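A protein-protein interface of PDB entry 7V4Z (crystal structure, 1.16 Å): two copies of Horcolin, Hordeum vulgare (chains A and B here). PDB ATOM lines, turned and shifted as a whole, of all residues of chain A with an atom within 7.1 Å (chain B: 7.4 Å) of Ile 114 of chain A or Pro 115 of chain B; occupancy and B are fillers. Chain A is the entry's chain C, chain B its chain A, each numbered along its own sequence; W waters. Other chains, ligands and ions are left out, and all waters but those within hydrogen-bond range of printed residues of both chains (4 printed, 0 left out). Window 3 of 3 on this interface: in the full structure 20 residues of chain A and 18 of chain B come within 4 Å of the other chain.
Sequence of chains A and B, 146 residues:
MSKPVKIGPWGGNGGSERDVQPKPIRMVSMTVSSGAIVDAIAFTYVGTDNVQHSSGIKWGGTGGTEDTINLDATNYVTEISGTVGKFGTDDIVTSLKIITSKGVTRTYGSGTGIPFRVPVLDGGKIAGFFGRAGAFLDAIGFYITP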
ATOM      1  N   TRP A  10     -11.614  18.882  24.536  1.00  0.00           N
ATOM      2  CA  TRP A  10     -11.524  19.644  25.821  1.00  0.00           C
ATOM      3  C   TRP A  10     -11.017  18.692  26.885  1.00  0.00           C
ATOM      4  O   TRP A  10     -11.572  17.590  27.048  1.00  0.00           O
ATOM      5  CB  TRP A  10     -12.868  20.239  26.178  1.00  0.00           C
ATOM      6  CG  TRP A  10     -13.342  21.251  25.190  1.00  0.00           C
ATOM      7  CD1 TRP A  10     -13.149  22.598  25.233  1.00  0.00           C
ATOM      8  CD2 TRP A  10     -14.057  21.000  23.985  1.00  0.00           C
ATOM      9  NE1 TRP A  10     -13.628  23.171  24.096  1.00  0.00           N
ATOM     10  CE2 TRP A  10     -14.232  22.226  23.328  1.00  0.00           C
ATOM     11  CE3 TRP A  10     -14.603  19.868  23.370  1.00  0.00           C
ATOM     12  CZ2 TRP A  10     -14.903  22.341  22.119  1.00  0.00           C
ATOM     13  CZ3 TRP A  10     -15.248  20.013  22.150  1.00  0.00           C
ATOM     14  CH2 TRP A  10     -15.431  21.238  21.575  1.00  0.00           C
ATOM     15  N   GLY A  82     -19.367  20.345  30.174  1.00  0.00           N
ATOM     16  CA  GLY A  82     -18.584  19.685  31.213  1.00  0.00           C
ATOM     17  C   GLY A  82     -17.551  20.604  31.778  1.00  0.00           C
ATOM     18  O   GLY A  82     -17.587  21.837  31.547  1.00  0.00           O
ATOM     19  N   THR A  83     -16.649  20.042  32.557  1.00  0.00           N
ATOM     20  CA  THR A  83     -15.552  20.795  33.207  1.00  0.00           C
ATOM     21  C   THR A  83     -14.251  20.038  33.004  1.00  0.00           C
ATOM     22  O   THR A  83     -14.241  18.792  33.019  1.00  0.00           O
ATOM     23  CB  THR A  83     -15.836  21.068  34.665  1.00  0.00           C
ATOM     24  OG1 THR A  83     -16.152  19.872  35.380  1.00  0.00           O
ATOM     25  CG2 THR A  83     -16.983  22.037  34.856  1.00  0.00           C
ATOM     26  N   VAL A  84     -13.185  20.819  32.934  1.00  0.00           N
ATOM     27  CA  VAL A  84     -11.805  20.289  32.905  1.00  0.00           C
ATOM     28  C   VAL A  84     -11.114  20.731  34.177  1.00  0.00           C
ATOM     29  O   VAL A  84     -11.022  21.947  34.450  1.00  0.00           O
ATOM     30  CB  VAL A  84     -11.053  20.773  31.664  1.00  0.00           C
ATOM     31  CG1 VAL A  84      -9.613  20.319  31.719  1.00  0.00           C
ATOM     32  CG2 VAL A  84     -11.735  20.290  30.383  1.00  0.00           C
ATOM     33  N   GLY A  85     -10.647  19.791  34.957  1.00  0.00           N
ATOM     34  CA  GLY A  85     -10.053  20.099  36.238  1.00  0.00           C
ATOM     35  C   GLY A  85      -9.015  19.078  36.594  1.00  0.00           C
ATOM     36  O   GLY A  85      -8.859  18.062  35.943  1.00  0.00           O
ATOM     37  N   THR A  94     -13.761  16.318  34.483  1.00  0.00           N
ATOM     38  CA  THR A  94     -14.216  16.152  35.858  1.00  0.00           C
ATOM     39  C   THR A  94     -15.731  16.091  36.001  1.00  0.00           C
ATOM     40  O   THR A  94     -16.260  15.659  37.055  1.00  0.00           O
ATOM     41  CB  THR A  94     -13.599  17.187  36.785  1.00  0.00           C
ATOM     42  OG1 THR A  94     -13.963  18.465  36.281  1.00  0.00           O
ATOM     43  CG2 THR A  94     -12.109  17.027  36.930  1.00  0.00           C
ATOM     44  N   THR A 112     -15.377  19.777  39.244  1.00  0.00           N
ATOM     45  CA  THR A 112     -15.383  21.211  38.915  1.00  0.00           C
ATOM     46  C   THR A 112     -14.228  21.528  37.973  1.00  0.00           C
ATOM     47  O   THR A 112     -13.319  20.685  37.708  1.00  0.00           O
ATOM     48  CB  THR A 112     -15.354  22.020  40.220  1.00  0.00           C
ATOM     49  OG1 THR A 112     -14.210  21.601  40.986  1.00  0.00           O
ATOM     50  CG2 THR A 112     -16.564  21.832  41.128  1.00  0.00           C
ATOM     51  N   GLY A 113     -14.167  22.755  37.503  1.00  0.00           N
ATOM     52  CA  GLY A 113     -13.051  23.236  36.691  1.00  0.00           C
ATOM     53  C   GLY A 113     -13.505  24.164  35.589  1.00  0.00           C
ATOM     54  O   GLY A 113     -14.574  24.813  35.693  1.00  0.00           O
ATOM     55  N   ILE A 114     -12.721  24.211  34.553  1.00  0.00           N
ATOM     56  CA  ILE A 114     -12.954  25.206  33.465  1.00  0.00           C
ATOM     57  C   ILE A 114     -14.043  24.652  32.571  1.00  0.00           C
ATOM     58  O   ILE A 114     -13.951  23.519  32.072  1.00  0.00           O
ATOM     59  CB  ILE A 114     -11.693  25.410  32.665  1.00  0.00           C
ATOM     60  CG1 ILE A 114     -10.570  25.865  33.627  1.00  0.00           C
ATOM     61  CG2 ILE A 114     -11.963  26.436  31.549  1.00  0.00           C
ATOM     62  CD1 ILE A 114      -9.308  26.444  33.123  1.00  0.00           C
ATOM     63  N   PRO A 115     -15.158  25.399  32.397  1.00  0.00           N
ATOM     64  CA  PRO A 115     -16.326  24.844  31.702  1.00  0.00           C
ATOM     65  C   PRO A 115     -16.140  24.853  30.194  1.00  0.00           C
ATOM     66  O   PRO A 115     -15.521  25.788  29.627  1.00  0.00           O
ATOM     67  CB  PRO A 115     -17.467  25.780  32.100  1.00  0.00           C
ATOM     68  CG  PRO A 115     -16.750  27.105  32.327  1.00  0.00           C
ATOM     69  CD  PRO A 115     -15.406  26.747  32.942  1.00  0.00           C
ATOM     70  N   PHE A 116     -16.760  23.885  29.545  1.00  0.00           N
ATOM     71  CA  PHE A 116     -16.964  23.859  28.088  1.00  0.00           C
ATOM     72  C   PHE A 116     -18.407  23.498  27.833  1.00  0.00           C
ATOM     73  O   PHE A 116     -19.030  22.774  28.629  1.00  0.00           O
ATOM     74  CB  PHE A 116     -16.011  22.930  27.379  1.00  0.00           C
ATOM     75  CG  PHE A 116     -16.140  21.462  27.758  1.00  0.00           C
ATOM     76  CD1 PHE A 116     -16.968  20.588  27.078  1.00  0.00           C
ATOM     77  CD2 PHE A 116     -15.389  20.951  28.811  1.00  0.00           C
ATOM     78  CE1 PHE A 116     -17.082  19.261  27.490  1.00  0.00           C
ATOM     79  CE2 PHE A 116     -15.467  19.621  29.173  1.00  0.00           C
ATOM     80  CZ  PHE A 116     -16.317  18.783  28.519  1.00  0.00           C
ATOM     81  N   ARG A 117     -18.953  24.011  26.744  1.00  0.00           N
ATOM     82  CA  ARG A 117     -20.364  23.747  26.385  1.00  0.00           C
ATOM     83  C   ARG A 117     -20.479  23.846  24.885  1.00  0.00           C
ATOM     84  O   ARG A 117     -20.077  24.857  24.290  1.00  0.00           O
ATOM     85  CB  ARG A 117     -21.264  24.750  27.087  1.00  0.00           C
ATOM     86  CG  ARG A 117     -22.764  24.689  26.752  1.00  0.00           C
ATOM     87  CD  ARG A 117     -23.451  25.666  27.700  1.00  0.00           C
ATOM     88  NE  ARG A 117     -24.853  25.643  27.332  1.00  0.00           N
ATOM     89  CZ  ARG A 117     -25.447  26.571  26.598  1.00  0.00           C
ATOM     90  NH1 ARG A 117     -26.731  26.417  26.284  1.00  0.00           N
ATOM     91  NH2 ARG A 117     -24.756  27.624  26.193  1.00  0.00           N
ATOM     92  N   TRP B  10     -22.057  31.444  22.421  1.00  0.00           N
ATOM     93  CA  TRP B  10     -21.347  31.699  23.700  1.00  0.00           C
ATOM     94  C   TRP B  10     -21.478  33.189  23.977  1.00  0.00           C
ATOM     95  O   TRP B  10     -21.145  34.020  23.109  1.00  0.00           O
ATOM     96  CB  TRP B  10     -19.876  31.301  23.542  1.00  0.00           C
ATOM     97  CG  TRP B  10     -19.696  29.821  23.393  1.00  0.00           C
ATOM     98  CD1 TRP B  10     -19.481  28.916  24.399  1.00  0.00           C
ATOM     99  CD2 TRP B  10     -19.797  29.056  22.194  1.00  0.00           C
ATOM    100  NE1 TRP B  10     -19.463  27.653  23.903  1.00  0.00           N
ATOM    101  CE2 TRP B  10     -19.650  27.684  22.555  1.00  0.00           C
ATOM    102  CE3 TRP B  10     -19.984  29.354  20.850  1.00  0.00           C
ATOM    103  CZ2 TRP B  10     -19.747  26.646  21.631  1.00  0.00           C
ATOM    104  CZ3 TRP B  10     -20.035  28.317  19.944  1.00  0.00           C
ATOM    105  CH2 TRP B  10     -19.925  26.993  20.318  1.00  0.00           C
ATOM    106  N   SER B  81     -11.569  31.197  19.643  1.00  0.00           N
ATOM    107  CA  SER B  81     -11.719  31.125  21.102  1.00  0.00           C
ATOM    108  C   SER B  81     -12.049  32.510  21.605  1.00  0.00           C
ATOM    109  O   SER B  81     -12.010  33.496  20.854  1.00  0.00           O
ATOM    110  CB  SER B  81     -10.467  30.580  21.710  1.00  0.00           C
ATOM    111  OG  SER B  81      -9.319  31.361  21.441  1.00  0.00           O
ATOM    112  N   GLY B  82     -12.355  32.609  22.885  1.00  0.00           N
ATOM    113  CA  GLY B  82     -12.658  33.931  23.433  1.00  0.00           C
ATOM    114  C   GLY B  82     -13.055  33.812  24.875  1.00  0.00           C
ATOM    115  O   GLY B  82     -12.820  32.792  25.516  1.00  0.00           O
ATOM    116  N   THR B  83     -13.624  34.877  25.380  1.00  0.00           N
ATOM    117  CA  THR B  83     -14.111  34.947  26.761  1.00  0.00           C
ATOM    118  C   THR B  83     -15.459  35.602  26.812  1.00  0.00           C
ATOM    119  O   THR B  83     -15.761  36.496  26.000  1.00  0.00           O
ATOM    120  CB  THR B  83     -13.118  35.679  27.695  1.00  0.00           C
ATOM    121  OG1 THR B  83     -12.768  36.934  27.143  1.00  0.00           O
ATOM    122  CG2 THR B  83     -11.850  34.883  27.938  1.00  0.00           C
ATOM    123  N   VAL B  84     -16.274  35.157  27.762  1.00  0.00           N
ATOM    124  CA  VAL B  84     -17.604  35.749  28.067  1.00  0.00           C
ATOM    125  C   VAL B  84     -17.513  36.303  29.485  1.00  0.00           C
ATOM    126  O   VAL B  84     -17.179  35.569  30.415  1.00  0.00           O
ATOM    127  CB  VAL B  84     -18.714  34.723  27.948  1.00  0.00           C
ATOM    128  CG1 VAL B  84     -20.016  35.309  28.395  1.00  0.00           C
ATOM    129  CG2 VAL B  84     -18.790  34.163  26.549  1.00  0.00           C
ATOM    130  N   SER B  95     -13.535  39.005  24.676  1.00  0.00           N
ATOM    131  CA  SER B  95     -12.390  38.765  23.796  1.00  0.00           C
ATOM    132  C   SER B  95     -12.717  37.714  22.773  1.00  0.00           C
ATOM    133  O   SER B  95     -13.583  36.868  22.984  1.00  0.00           O
ATOM    134  CB  SER B  95     -11.123  38.430  24.513  1.00  0.00           C
ATOM    135  OG  SER B  95     -11.136  37.086  25.001  1.00  0.00           O
ATOM    136  N   THR B 112     -11.522  38.830  30.069  1.00  0.00           N
ATOM    137  CA  THR B 112     -12.204  38.874  31.341  1.00  0.00           C
ATOM    138  C   THR B 112     -13.418  37.936  31.322  1.00  0.00           C
ATOM    139  O   THR B 112     -14.247  37.996  30.406  1.00  0.00           O
ATOM    140  CB  THR B 112     -12.442  40.327  31.702  1.00  0.00           C
ATOM    141  OG1 THR B 112     -12.809  40.266  33.083  1.00  0.00           O
ATOM    142  CG2 THR B 112     -13.424  41.009  30.788  1.00  0.00           C
ATOM    143  N   GLY B 113     -13.491  37.033  32.260  1.00  0.00           N
ATOM    144  CA  GLY B 113     -14.606  36.093  32.368  1.00  0.00           C
ATOM    145  C   GLY B 113     -14.218  34.665  32.118  1.00  0.00           C
ATOM    146  O   GLY B 113     -13.155  34.200  32.572  1.00  0.00           O
ATOM    147  N   ILE B 114     -15.067  33.947  31.441  1.00  0.00           N
ATOM    148  CA  ILE B 114     -14.970  32.486  31.289  1.00  0.00           C
ATOM    149  C   ILE B 114     -14.625  32.189  29.845  1.00  0.00           C
ATOM    150  O   ILE B 114     -15.269  32.686  28.906  1.00  0.00           O
ATOM    151  CB  ILE B 114     -16.355  31.865  31.626  1.00  0.00           C
ATOM    152  CG1 ILE B 114     -16.779  32.217  33.044  1.00  0.00           C
ATOM    153  CG2 ILE B 114     -16.353  30.350  31.371  1.00  0.00           C
ATOM    154  CD1 ILE B 114     -18.060  31.576  33.576  1.00  0.00           C
ATOM    155  N   PRO B 115     -13.602  31.344  29.597  1.00  0.00           N
ATOM    156  CA  PRO B 115     -13.143  31.078  28.258  1.00  0.00           C
ATOM    157  C   PRO B 115     -14.049  30.072  27.530  1.00  0.00           C
ATOM    158  O   PRO B 115     -14.596  29.155  28.152  1.00  0.00           O
ATOM    159  CB  PRO B 115     -11.749  30.511  28.474  1.00  0.00           C
ATOM    160  CG  PRO B 115     -11.837  29.814  29.782  1.00  0.00           C
ATOM    161  CD  PRO B 115     -12.745  30.696  30.614  1.00  0.00           C
ATOM    162  N   PHE B 116     -14.039  30.184  26.219  1.00  0.00           N
ATOM    163  CA  PHE B 116     -14.558  29.158  25.292  1.00  0.00           C
ATOM    164  C   PHE B 116     -13.542  28.970  24.193  1.00  0.00           C
ATOM    165  O   PHE B 116     -12.804  29.906  23.809  1.00  0.00           O
ATOM    166  CB  PHE B 116     -15.950  29.524  24.758  1.00  0.00           C
ATOM    167  CG  PHE B 116     -15.973  30.757  23.889  1.00  0.00           C
ATOM    168  CD1 PHE B 116     -15.830  30.669  22.504  1.00  0.00           C
ATOM    169  CD2 PHE B 116     -16.191  32.011  24.417  1.00  0.00           C
ATOM    170  CE1 PHE B 116     -15.869  31.815  21.704  1.00  0.00           C
ATOM    171  CE2 PHE B 116     -16.260  33.134  23.618  1.00  0.00           C
ATOM    172  CZ  PHE B 116     -16.063  33.033  22.285  1.00  0.00           C
ATOM    173  N   ARG B 117     -13.571  27.793  23.580  1.00  0.00           N
ATOM    174  CA  ARG B 117     -12.706  27.502  22.419  1.00  0.00           C
ATOM    175  C   ARG B 117     -13.423  26.545  21.520  1.00  0.00           C
ATOM    176  O   ARG B 117     -13.928  25.502  22.011  1.00  0.00           O
ATOM    177  CB  ARG B 117     -11.351  27.046  22.863  1.00  0.00           C
ATOM    178  CG  ARG B 117     -11.256  25.758  23.547  1.00  0.00           C
ATOM    179  CD  ARG B 117      -9.736  25.359  23.500  1.00  0.00           C
ATOM    180  NE  ARG B 117      -9.414  24.046  24.013  1.00  0.00           N
ATOM    181  CZ  ARG B 117      -9.453  23.711  25.309  1.00  0.00           C
ATOM    182  NH1 ARG B 117      -9.858  24.601  26.196  1.00  0.00           N
ATOM    183  NH2 ARG B 117      -9.149  22.481  25.719  1.00  0.00           N
HETATM  184  O   HOH W   1     -17.400  26.250  25.774  1.00  0.00           O
HETATM  185  O   HOH W   2     -14.757  25.774  25.250  1.00  0.00           O
HETATM  186  O   HOH W   3     -22.200  27.539  24.439  1.00  0.00           O
HETATM  187  O   HOH W   4     -17.175  28.101  27.900  1.00  0.00           O
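Water W3 bridges the indole nitrogen (NE1) of Trp 10 of chain B (2.8 Å) and the guanidinium group (NH2) of Arg 117 of chain A (3.1 Å). Water W4 bridges O of Pro 115 of chain B (2.8 Å) and O of Pro 115 of chain A (3.3 Å). Water W2 bridges N of Arg 117 of chain B and NE1 of Trp 10 of chain A. Water W1 lies within hydrogen-bond range of the backbone NH of Arg 117 of chain A (2.9 Å) and the indole nitrogen of Trp 10 of chain B (3.1 Å).
Of the 12 printed residues of chain B, 4 touch a printed residue of chain A. Hydrophobic or aromatic side chains of chain B within 4 Å of the printed part of chain A: Trp 10, Ile 114 and Pro 115. Of the 12 printed residues of chain A, 4 touch a printed residue of chain B. Printed residues of chain A that touch a printed residue of chain B: Trp 10, Ile 114, Pro 115 and Arg 117. Hydrophobic or aromatic side chains of chain A within 4 Å of the printed part of chain B: Trp 10, Ile 114 and Pro 115. Among the printed residues, 5 pairs touch across the chains.
Ile 114 of chain A touches Pro 115 of chain B. Ile 114 of chain B touches Pro 115 of chain A. Pro 115 of chain A touches Pro 115 of chain B.
Of the printed residues of chain B, Trp 10 of chain A touches Arg 117. Ile 114 of chain A touches just one residue of chain B: Pro 115. Of the printed residues of chain B, Pro 115 of chain A touches Ile 114 and Pro 115. Gly 82 of chain B touches none of the printed residues of chain A. Thr 83 of chain B touches none of the printed residues of chain A. Of the printed residues of chain A, Ile 114 of chain B touches Pro 115. Of the printed residues of chain A, Pro 115 of chain B touches Ile 114 and Pro 115. Of the printed residues of chain A, Arg 117 of chain B touches Trp 10. The nearest residue of chain A that does not touch Pro 115 of chain B is Phe 116 of chain A (5.8 Å). The nearest printed residue of chain A that does not touch Trp 10 of chain B is Phe 116 of chain A (5.8 Å).
The indole nitrogen of Trp 10 of chain B lies within hydrogen-bond range of the backbone carbonyl oxygen of Arg 117 of chain A. O of Arg 117 of chain B sits at hydrogen-bond distance from NE1 of Trp 10 of chain A, at 3.1 Å.
The backbone NH (N) of Ile 114 of chain B sits at hydrogen-bond distance from the backbone carbonyl oxygen (O) of Val 84 of chain B (2.9 Å). N of Ile 114 of chain A sits at hydrogen-bond distance from O of Val 84 of chain A (2.8 Å).
Trp 10 of chain A touches Arg 117 of chain B, and with the chains exchanged Arg 117 of chain A touches Trp 10 of chain B. Ile 114 of chain A touches Pro 115 of chain B, and with the chains exchanged Pro 115 of chain A touches Ile 114 of chain B. Pro 115 of chain B touches its own counterpart, Pro 115 of chain A. 10 positions are printed for both chains.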
